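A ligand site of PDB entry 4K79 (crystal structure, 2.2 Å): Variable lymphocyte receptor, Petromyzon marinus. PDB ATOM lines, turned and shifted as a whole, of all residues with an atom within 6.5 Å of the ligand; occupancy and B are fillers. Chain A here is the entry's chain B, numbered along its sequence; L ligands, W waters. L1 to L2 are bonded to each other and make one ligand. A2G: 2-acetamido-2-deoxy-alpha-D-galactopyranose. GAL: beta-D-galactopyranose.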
ATOM      1  N   HIS A  60      -1.091 -15.550   3.103  1.00  0.00           N
ATOM      2  CA  HIS A  60      -1.351 -16.594   4.069  1.00  0.00           C
ATOM      3  C   HIS A  60      -0.108 -16.943   4.894  1.00  0.00           C
ATOM      4  O   HIS A  60       0.782 -17.681   4.420  1.00  0.00           O
ATOM      5  CB  HIS A  60      -1.747 -17.820   3.366  1.00  0.00           C
ATOM      6  CG  HIS A  60      -3.044 -17.695   2.643  1.00  0.00           C
ATOM      7  ND1 HIS A  60      -3.208 -16.877   1.544  1.00  0.00           N
ATOM      8  CD2 HIS A  60      -4.234 -18.293   2.850  1.00  0.00           C
ATOM      9  CE1 HIS A  60      -4.438 -17.014   1.088  1.00  0.00           C
ATOM     10  NE2 HIS A  60      -5.081 -17.877   1.854  1.00  0.00           N
ATOM     11  N   TRP A  62      -0.523 -18.060   8.150  1.00  0.00           N
ATOM     12  CA  TRP A  62      -1.009 -18.764   9.284  1.00  0.00           C
ATOM     13  C   TRP A  62      -0.258 -20.074   9.554  1.00  0.00           C
ATOM     14  O   TRP A  62       0.268 -20.709   8.640  1.00  0.00           O
ATOM     15  CB  TRP A  62      -2.515 -18.964   9.182  1.00  0.00           C
ATOM     16  CG  TRP A  62      -2.966 -19.802   8.050  1.00  0.00           C
ATOM     17  CD1 TRP A  62      -3.344 -19.391   6.840  1.00  0.00           C
ATOM     18  CD2 TRP A  62      -3.081 -21.222   8.056  1.00  0.00           C
ATOM     19  NE1 TRP A  62      -3.686 -20.442   6.066  1.00  0.00           N
ATOM     20  CE2 TRP A  62      -3.556 -21.595   6.779  1.00  0.00           C
ATOM     21  CE3 TRP A  62      -2.858 -22.220   9.017  1.00  0.00           C
ATOM     22  CZ2 TRP A  62      -3.823 -22.920   6.417  1.00  0.00           C
ATOM     23  CZ3 TRP A  62      -3.106 -23.562   8.671  1.00  0.00           C
ATOM     24  CH2 TRP A  62      -3.594 -23.887   7.380  1.00  0.00           C
ATOM     25  N   GLY A  63      -0.188 -20.432  10.842  1.00  0.00           N
ATOM     26  CA  GLY A  63       0.449 -21.670  11.279  1.00  0.00           C
ATOM     27  C   GLY A  63       1.943 -21.664  11.122  1.00  0.00           C
ATOM     28  O   GLY A  63       2.504 -22.629  10.642  1.00  0.00           O
ATOM     29  N   TRP A  84      -3.749 -13.393   6.669  1.00  0.00           N
ATOM     30  CA  TRP A  84      -3.992 -14.475   7.630  1.00  0.00           C
ATOM     31  C   TRP A  84      -2.771 -14.747   8.459  1.00  0.00           C
ATOM     32  O   TRP A  84      -1.807 -15.294   7.950  1.00  0.00           O
ATOM     33  CB  TRP A  84      -4.373 -15.771   6.910  1.00  0.00           C
ATOM     34  CG  TRP A  84      -5.575 -15.638   6.088  1.00  0.00           C
ATOM     35  CD1 TRP A  84      -5.659 -15.718   4.739  1.00  0.00           C
ATOM     36  CD2 TRP A  84      -6.894 -15.383   6.563  1.00  0.00           C
ATOM     37  NE1 TRP A  84      -6.968 -15.541   4.332  1.00  0.00           N
ATOM     38  CE2 TRP A  84      -7.745 -15.356   5.437  1.00  0.00           C
ATOM     39  CE3 TRP A  84      -7.450 -15.201   7.835  1.00  0.00           C
ATOM     40  CZ2 TRP A  84      -9.109 -15.145   5.531  1.00  0.00           C
ATOM     41  CZ3 TRP A  84      -8.800 -14.977   7.943  1.00  0.00           C
ATOM     42  CH2 TRP A  84      -9.627 -14.948   6.802  1.00  0.00           C
ATOM     43  N   LEU A  85      -2.814 -14.313   9.731  1.00  0.00           N
ATOM     44  CA  LEU A  85      -1.697 -14.474  10.657  1.00  0.00           C
ATOM     45  C   LEU A  85      -1.999 -15.467  11.767  1.00  0.00           C
ATOM     46  O   LEU A  85      -1.216 -15.612  12.693  1.00  0.00           O
ATOM     47  CB  LEU A  85      -1.363 -13.118  11.282  1.00  0.00           C
ATOM     48  CG  LEU A  85      -0.643 -12.141  10.348  1.00  0.00           C
ATOM     49  CD1 LEU A  85      -0.903 -10.732  10.815  1.00  0.00           C
ATOM     50  CD2 LEU A  85       0.899 -12.485  10.371  1.00  0.00           C
ATOM     51  N   ASN A  86      -3.161 -16.124  11.683  1.00  0.00           N
ATOM     52  CA  ASN A  86      -3.619 -17.020  12.733  1.00  0.00           C
ATOM     53  C   ASN A  86      -2.542 -18.038  13.111  1.00  0.00           C
ATOM     54  O   ASN A  86      -1.775 -18.486  12.244  1.00  0.00           O
ATOM     55  CB  ASN A  86      -4.854 -17.803  12.302  1.00  0.00           C
ATOM     56  CG  ASN A  86      -5.836 -16.961  11.516  1.00  0.00           C
ATOM     57  OD1 ASN A  86      -5.729 -16.839  10.285  1.00  0.00           O
ATOM     58  ND2 ASN A  86      -6.828 -16.421  12.183  1.00  0.00           N
ATOM     59  N   SER A  87      -2.540 -18.438  14.362  1.00  0.00           N
ATOM     60  CA  SER A  87      -1.708 -19.545  14.856  1.00  0.00           C
ATOM     61  C   SER A  87      -0.256 -19.305  14.645  1.00  0.00           C
ATOM     62  O   SER A  87       0.478 -20.138  14.103  1.00  0.00           O
ATOM     63  CB  SER A  87      -2.115 -20.881  14.224  1.00  0.00           C
ATOM     64  OG  SER A  87      -3.510 -20.989  14.252  1.00  0.00           O
ATOM     65  N   LEU A 107      -9.023 -10.065   7.983  1.00  0.00           N
ATOM     66  CA  LEU A 107      -7.813 -10.017   8.786  1.00  0.00           C
ATOM     67  C   LEU A 107      -7.941 -11.047   9.887  1.00  0.00           C
ATOM     68  O   LEU A 107      -8.873 -10.976  10.718  1.00  0.00           O
ATOM     69  CB  LEU A 107      -7.597  -8.609   9.350  1.00  0.00           C
ATOM     70  CG  LEU A 107      -6.484  -8.441  10.395  1.00  0.00           C
ATOM     71  CD1 LEU A 107      -5.096  -8.971   9.888  1.00  0.00           C
ATOM     72  CD2 LEU A 107      -6.442  -7.003  10.803  1.00  0.00           C
ATOM     73  N   GLY A 108      -7.038 -12.036   9.852  1.00  0.00           N
ATOM     74  CA  GLY A 108      -7.042 -13.063  10.870  1.00  0.00           C
ATOM     75  C   GLY A 108      -5.872 -12.942  11.837  1.00  0.00           C
ATOM     76  O   GLY A 108      -4.709 -12.931  11.455  1.00  0.00           O
ATOM     77  N   LEU A 109      -6.233 -12.905  13.118  1.00  0.00           N
ATOM     78  CA  LEU A 109      -5.271 -12.747  14.188  1.00  0.00           C
ATOM     79  C   LEU A 109      -5.552 -13.694  15.354  1.00  0.00           C
ATOM     80  O   LEU A 109      -5.204 -13.334  16.476  1.00  0.00           O
ATOM     81  CB  LEU A 109      -5.293 -11.264  14.662  1.00  0.00           C
ATOM     82  CG  LEU A 109      -4.861 -10.157  13.676  1.00  0.00           C
ATOM     83  CD1 LEU A 109      -5.251  -8.794  14.194  1.00  0.00           C
ATOM     84  CD2 LEU A 109      -3.367 -10.175  13.447  1.00  0.00           C
ATOM     85  N   CYS A 110      -6.170 -14.900  15.121  1.00  0.00           N
ATOM     86  CA  CYS A 110      -6.617 -15.751  16.224  1.00  0.00           C
ATOM     87  C   CYS A 110      -5.453 -16.590  16.736  1.00  0.00           C
ATOM     88  O   CYS A 110      -4.444 -16.754  16.070  1.00  0.00           O
ATOM     89  CB  CYS A 110      -7.771 -16.675  15.805  1.00  0.00           C
ATOM     90  SG  CYS A 110      -7.237 -18.168  14.860  1.00  0.00           S
ATOM     91  N   CYS A 111      -5.636 -17.201  17.892  1.00  0.00           N
ATOM     92  CA  CYS A 111      -4.885 -18.417  18.233  1.00  0.00           C
ATOM     93  C   CYS A 111      -3.417 -18.117  18.427  1.00  0.00           C
ATOM     94  O   CYS A 111      -2.575 -18.860  17.983  1.00  0.00           O
ATOM     95  CB  CYS A 111      -5.090 -19.454  17.102  1.00  0.00           C
ATOM     96  SG  CYS A 111      -6.859 -19.561  16.491  1.00  0.00           S
ATOM     97  N   GLN A 130     -14.178  -8.888   7.813  1.00  0.00           N
ATOM     98  CA  GLN A 130     -14.063 -10.014   8.739  1.00  0.00           C
ATOM     99  C   GLN A 130     -12.800  -9.875   9.574  1.00  0.00           C
ATOM    100  O   GLN A 130     -11.720  -9.661   9.024  1.00  0.00           O
ATOM    101  CB  GLN A 130     -14.013 -11.314   7.960  1.00  0.00           C
ATOM    102  CG  GLN A 130     -15.237 -11.558   7.115  1.00  0.00           C
ATOM    103  CD  GLN A 130     -15.425 -13.026   6.940  1.00  0.00           C
ATOM    104  OE1 GLN A 130     -14.606 -13.801   7.458  1.00  0.00           O
ATOM    105  NE2 GLN A 130     -16.453 -13.441   6.206  1.00  0.00           N
ATOM    106  N   LEU A 131     -12.954  -9.970  10.896  1.00  0.00           N
ATOM    107  CA  LEU A 131     -11.859  -9.821  11.813  1.00  0.00           C
ATOM    108  C   LEU A 131     -11.853 -10.925  12.877  1.00  0.00           C
ATOM    109  O   LEU A 131     -12.800 -11.050  13.675  1.00  0.00           O
ATOM    110  CB  LEU A 131     -12.003  -8.477  12.485  1.00  0.00           C
ATOM    111  CG  LEU A 131     -10.957  -8.106  13.553  1.00  0.00           C
ATOM    112  CD1 LEU A 131      -9.523  -8.206  13.022  1.00  0.00           C
ATOM    113  CD2 LEU A 131     -11.262  -6.722  14.051  1.00  0.00           C
ATOM    114  N   GLY A 132     -10.784 -11.708  12.891  1.00  0.00           N
ATOM    115  CA  GLY A 132     -10.626 -12.807  13.837  1.00  0.00           C
ATOM    116  C   GLY A 132      -9.628 -12.470  14.955  1.00  0.00           C
ATOM    117  O   GLY A 132      -8.418 -12.346  14.696  1.00  0.00           O
ATOM    118  N   LEU A 133     -10.159 -12.317  16.182  1.00  0.00           N
ATOM    119  CA  LEU A 133      -9.348 -12.031  17.409  1.00  0.00           C
ATOM    120  C   LEU A 133      -9.456 -13.121  18.464  1.00  0.00           C
ATOM    121  O   LEU A 133      -8.901 -13.007  19.568  1.00  0.00           O
ATOM    122  CB  LEU A 133      -9.824 -10.716  18.010  1.00  0.00           C
ATOM    123  CG  LEU A 133      -9.377  -9.552  17.140  1.00  0.00           C
ATOM    124  CD1 LEU A 133     -10.056  -8.262  17.567  1.00  0.00           C
ATOM    125  CD2 LEU A 133      -7.853  -9.392  17.195  1.00  0.00           C
ATOM    126  N   ASP A 134     -10.165 -14.202  18.146  1.00  0.00           N
ATOM    127  CA  ASP A 134     -10.385 -15.272  19.091  1.00  0.00           C
ATOM    128  C   ASP A 134      -9.085 -15.984  19.522  1.00  0.00           C
ATOM    129  O   ASP A 134      -8.084 -15.991  18.790  1.00  0.00           O
ATOM    130  CB  ASP A 134     -11.366 -16.261  18.468  1.00  0.00           C
ATOM    131  CG  ASP A 134     -10.916 -16.705  17.069  1.00  0.00           C
ATOM    132  OD1 ASP A 134     -10.797 -15.850  16.153  1.00  0.00           O
ATOM    133  OD2 ASP A 134     -10.672 -17.913  16.884  1.00  0.00           O
ATOM    134  N   GLN A 135      -9.141 -16.628  20.689  1.00  0.00           N
ATOM    135  CA  GLN A 135      -8.057 -17.519  21.171  1.00  0.00           C
ATOM    136  C   GLN A 135      -6.727 -16.815  21.348  1.00  0.00           C
ATOM    137  O   GLN A 135      -5.681 -17.259  20.868  1.00  0.00           O
ATOM    138  CB  GLN A 135      -7.918 -18.761  20.291  1.00  0.00           C
ATOM    139  CG  GLN A 135      -9.242 -19.387  20.043  1.00  0.00           C
ATOM    140  CD  GLN A 135      -9.154 -20.568  19.119  1.00  0.00           C
ATOM    141  OE1 GLN A 135      -8.492 -21.564  19.436  1.00  0.00           O
ATOM    142  NE2 GLN A 135      -9.823 -20.457  17.964  1.00  0.00           N
ATOM    143  N   TRP A 156     -14.777 -12.431  15.529  1.00  0.00           N
ATOM    144  CA  TRP A 156     -14.556 -13.543  16.439  1.00  0.00           C
ATOM    145  C   TRP A 156     -13.800 -12.994  17.609  1.00  0.00           C
ATOM    146  O   TRP A 156     -12.720 -12.339  17.436  1.00  0.00           O
ATOM    147  CB  TRP A 156     -13.638 -14.576  15.821  1.00  0.00           C
ATOM    148  CG  TRP A 156     -14.161 -15.432  14.732  1.00  0.00           C
ATOM    149  CD1 TRP A 156     -14.427 -16.799  14.815  1.00  0.00           C
ATOM    150  CD2 TRP A 156     -14.389 -15.069  13.365  1.00  0.00           C
ATOM    151  NE1 TRP A 156     -14.846 -17.273  13.583  1.00  0.00           N
ATOM    152  CE2 TRP A 156     -14.816 -16.248  12.674  1.00  0.00           C
ATOM    153  CE3 TRP A 156     -14.263 -13.871  12.642  1.00  0.00           C
ATOM    154  CZ2 TRP A 156     -15.157 -16.253  11.313  1.00  0.00           C
ATOM    155  CZ3 TRP A 156     -14.580 -13.883  11.266  1.00  0.00           C
ATOM    156  CH2 TRP A 156     -15.040 -15.065  10.629  1.00  0.00           C
ATOM    157  N   HIS A 158     -14.268 -14.861  20.983  1.00  0.00           N
ATOM    158  CA  HIS A 158     -14.245 -15.893  22.019  1.00  0.00           C
ATOM    159  C   HIS A 158     -12.858 -16.373  22.417  1.00  0.00           C
ATOM    160  O   HIS A 158     -11.860 -16.073  21.774  1.00  0.00           O
ATOM    161  CB  HIS A 158     -15.098 -17.059  21.573  1.00  0.00           C
ATOM    162  CG  HIS A 158     -14.553 -17.775  20.376  1.00  0.00           C
ATOM    163  ND1 HIS A 158     -13.641 -18.807  20.498  1.00  0.00           N
ATOM    164  CD2 HIS A 158     -14.745 -17.586  19.049  1.00  0.00           C
ATOM    165  CE1 HIS A 158     -13.303 -19.228  19.287  1.00  0.00           C
ATOM    166  NE2 HIS A 158     -13.970 -18.509  18.395  1.00  0.00           N
ATOM    167  N   GLU A 185     -18.413 -17.517  15.683  1.00  0.00           N
ATOM    168  CA  GLU A 185     -17.483 -18.629  15.995  1.00  0.00           C
ATOM    169  C   GLU A 185     -17.395 -19.520  14.769  1.00  0.00           C
ATOM    170  O   GLU A 185     -18.331 -19.541  13.973  1.00  0.00           O
ATOM    171  CB  GLU A 185     -18.099 -19.420  17.160  1.00  0.00           C
ATOM    172  CG  GLU A 185     -17.553 -20.807  17.463  1.00  0.00           C
ATOM    173  CD  GLU A 185     -18.147 -21.398  18.754  1.00  0.00           C
ATOM    174  OE1 GLU A 185     -19.230 -20.950  19.214  1.00  0.00           O
ATOM    175  OE2 GLU A 185     -17.487 -22.293  19.317  1.00  0.00           O
ATOM    176  N   GLY A 186     -16.288 -20.253  14.638  1.00  0.00           N
ATOM    177  CA  GLY A 186     -16.185 -21.294  13.613  1.00  0.00           C
ATOM    178  C   GLY A 186     -15.759 -20.770  12.240  1.00  0.00           C
ATOM    179  O   GLY A 186     -15.577 -19.562  12.046  1.00  0.00           O
ATOM    180  N   TRP A 187     -15.563 -21.683  11.308  1.00  0.00           N
ATOM    181  CA  TRP A 187     -15.014 -21.364   9.978  1.00  0.00           C
ATOM    182  C   TRP A 187     -15.731 -22.243   8.976  1.00  0.00           C
ATOM    183  O   TRP A 187     -15.569 -23.462   9.007  1.00  0.00           O
ATOM    184  CB  TRP A 187     -13.492 -21.592   9.933  1.00  0.00           C
ATOM    185  CG  TRP A 187     -12.909 -21.176   8.620  1.00  0.00           C
ATOM    186  CD1 TRP A 187     -12.393 -21.997   7.643  1.00  0.00           C
ATOM    187  CD2 TRP A 187     -12.831 -19.835   8.090  1.00  0.00           C
ATOM    188  NE1 TRP A 187     -11.988 -21.251   6.561  1.00  0.00           N
ATOM    189  CE2 TRP A 187     -12.252 -19.933   6.802  1.00  0.00           C
ATOM    190  CE3 TRP A 187     -13.173 -18.576   8.601  1.00  0.00           C
ATOM    191  CZ2 TRP A 187     -11.997 -18.791   6.009  1.00  0.00           C
ATOM    192  CZ3 TRP A 187     -12.936 -17.447   7.804  1.00  0.00           C
ATOM    193  CH2 TRP A 187     -12.352 -17.575   6.517  1.00  0.00           C
HETATM  194  O5  A2G L   1      -6.805 -20.404   7.439  1.00  0.00           O
HETATM  195  C1  A2G L   1      -6.712 -21.375   8.491  1.00  0.00           C
HETATM  196  O1  A2G L   1      -7.586 -22.486   8.226  1.00  0.00           O
HETATM  197  C2  A2G L   1      -7.116 -20.767   9.817  1.00  0.00           C
HETATM  198  N2  A2G L   1      -6.980 -21.762  10.881  1.00  0.00           N
HETATM  199  C3  A2G L   1      -8.573 -20.396   9.681  1.00  0.00           C
HETATM  200  O3  A2G L   1      -9.061 -19.852  10.925  1.00  0.00           O
HETATM  201  C4  A2G L   1      -8.782 -19.456   8.487  1.00  0.00           C
HETATM  202  O4  A2G L   1      -8.150 -18.224   8.816  1.00  0.00           O
HETATM  203  C5  A2G L   1      -8.150 -19.962   7.186  1.00  0.00           C
HETATM  204  C6  A2G L   1      -8.165 -18.848   6.151  1.00  0.00           C
HETATM  205  O6  A2G L   1      -7.857 -19.308   4.831  1.00  0.00           O
HETATM  206  C7  A2G L   1      -6.172 -21.676  11.944  1.00  0.00           C
HETATM  207  O7  A2G L   1      -5.519 -20.686  12.208  1.00  0.00           O
HETATM  208  C8  A2G L   1      -6.103 -22.891  12.818  1.00  0.00           C
HETATM  209  C1  GAL L   2     -10.181 -19.233  11.261  1.00  0.00           C
HETATM  210  C2  GAL L   2     -10.252 -19.592  12.741  1.00  0.00           C
HETATM  211  C3  GAL L   2     -11.411 -18.836  13.323  1.00  0.00           C
HETATM  212  C4  GAL L   2     -11.334 -17.336  12.956  1.00  0.00           C
HETATM  213  C5  GAL L   2     -11.021 -17.065  11.475  1.00  0.00           C
HETATM  214  C6  GAL L   2     -10.735 -15.582  11.242  1.00  0.00           C
HETATM  215  O2  GAL L   2     -10.560 -20.954  12.823  1.00  0.00           O
HETATM  216  O3  GAL L   2     -11.438 -19.123  14.709  1.00  0.00           O
HETATM  217  O4  GAL L   2     -10.362 -16.704  13.745  1.00  0.00           O
HETATM  218  O5  GAL L   2      -9.945 -17.859  10.996  1.00  0.00           O
HETATM  219  O6  GAL L   2      -9.422 -15.233  11.655  1.00  0.00           O
HETATM  220  O   HOH W   1     -13.841 -20.037  15.857  1.00  0.00           O
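The side-chain amide nitrogen of Asn 86 is in hydrogen-bond range of an oxygen (O6) of GAL L2, at 2.9 Å.
The side-chain sulfur (SG) of Cys 110 sits close to an oxygen (O4) of GAL L2 (3.6 Å).
The indole nitrogen (NE1) of Trp 62 sits at hydrogen-bond distance from an oxygen (O5) of A2G L1 (3.4 Å).
OD1 of Asp 134 is in hydrogen-bond range of O4 of GAL L2.
The side-chain hydroxyl (OG) of Ser 87 sits at hydrogen-bond distance from an oxygen (O7) of A2G L1, 2.9 Å away.
The indole nitrogen of Trp 156 sits at hydrogen-bond distance from the backbone carbonyl oxygen of Gly 186 (2.9 Å).
The side-chain sulfur of Cys 110 sits at hydrogen-bond distance from the side-chain amide nitrogen of Asn 86, at 3.2 Å.
The backbone carbonyl oxygen (O) of Asn 86 sits at hydrogen-bond distance from the backbone NH (N) of Gly 63.
O of Gly 132 sits at hydrogen-bond distance from N of Leu 109 (2.8 Å).
The backbone carbonyl oxygen of Trp 156 lies within hydrogen-bond range of the backbone NH of Leu 133 (2.9 Å).
SG of Cys 110 forms a disulfide with SG of Cys 111, at 2.2 Å.
The backbone NH of Cys 111 sits at hydrogen-bond distance from the backbone carbonyl oxygen of Gln 135 (3.0 Å).
The backbone carbonyl oxygen (O) of Leu 107 sits at hydrogen-bond distance from the backbone NH (N) of Gly 132, at 3.0 Å.
Residues that only touch the ligand: Trp 84 (3.3 Å), Gly 108 (3.3 Å), Gly 132 (3.5 Å), Trp 156 (3.6 Å), Trp 187 (3.8 Å) and Gln 135 (3.9 Å).
Hydrophobic or aromatic side chains that line the ligand: Trp 62, Trp 84, Trp 156 and Trp 187.
Of the 23 residues printed, 11 come within 4 Å of the ligand.
Water W1 lies within hydrogen-bond range of the backbone NH of Gly 186 (2.7 Å), an oxygen (O3) of GAL L2 (2.8 Å) and a ring nitrogen (NE2) of His 158 (3.0 Å).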
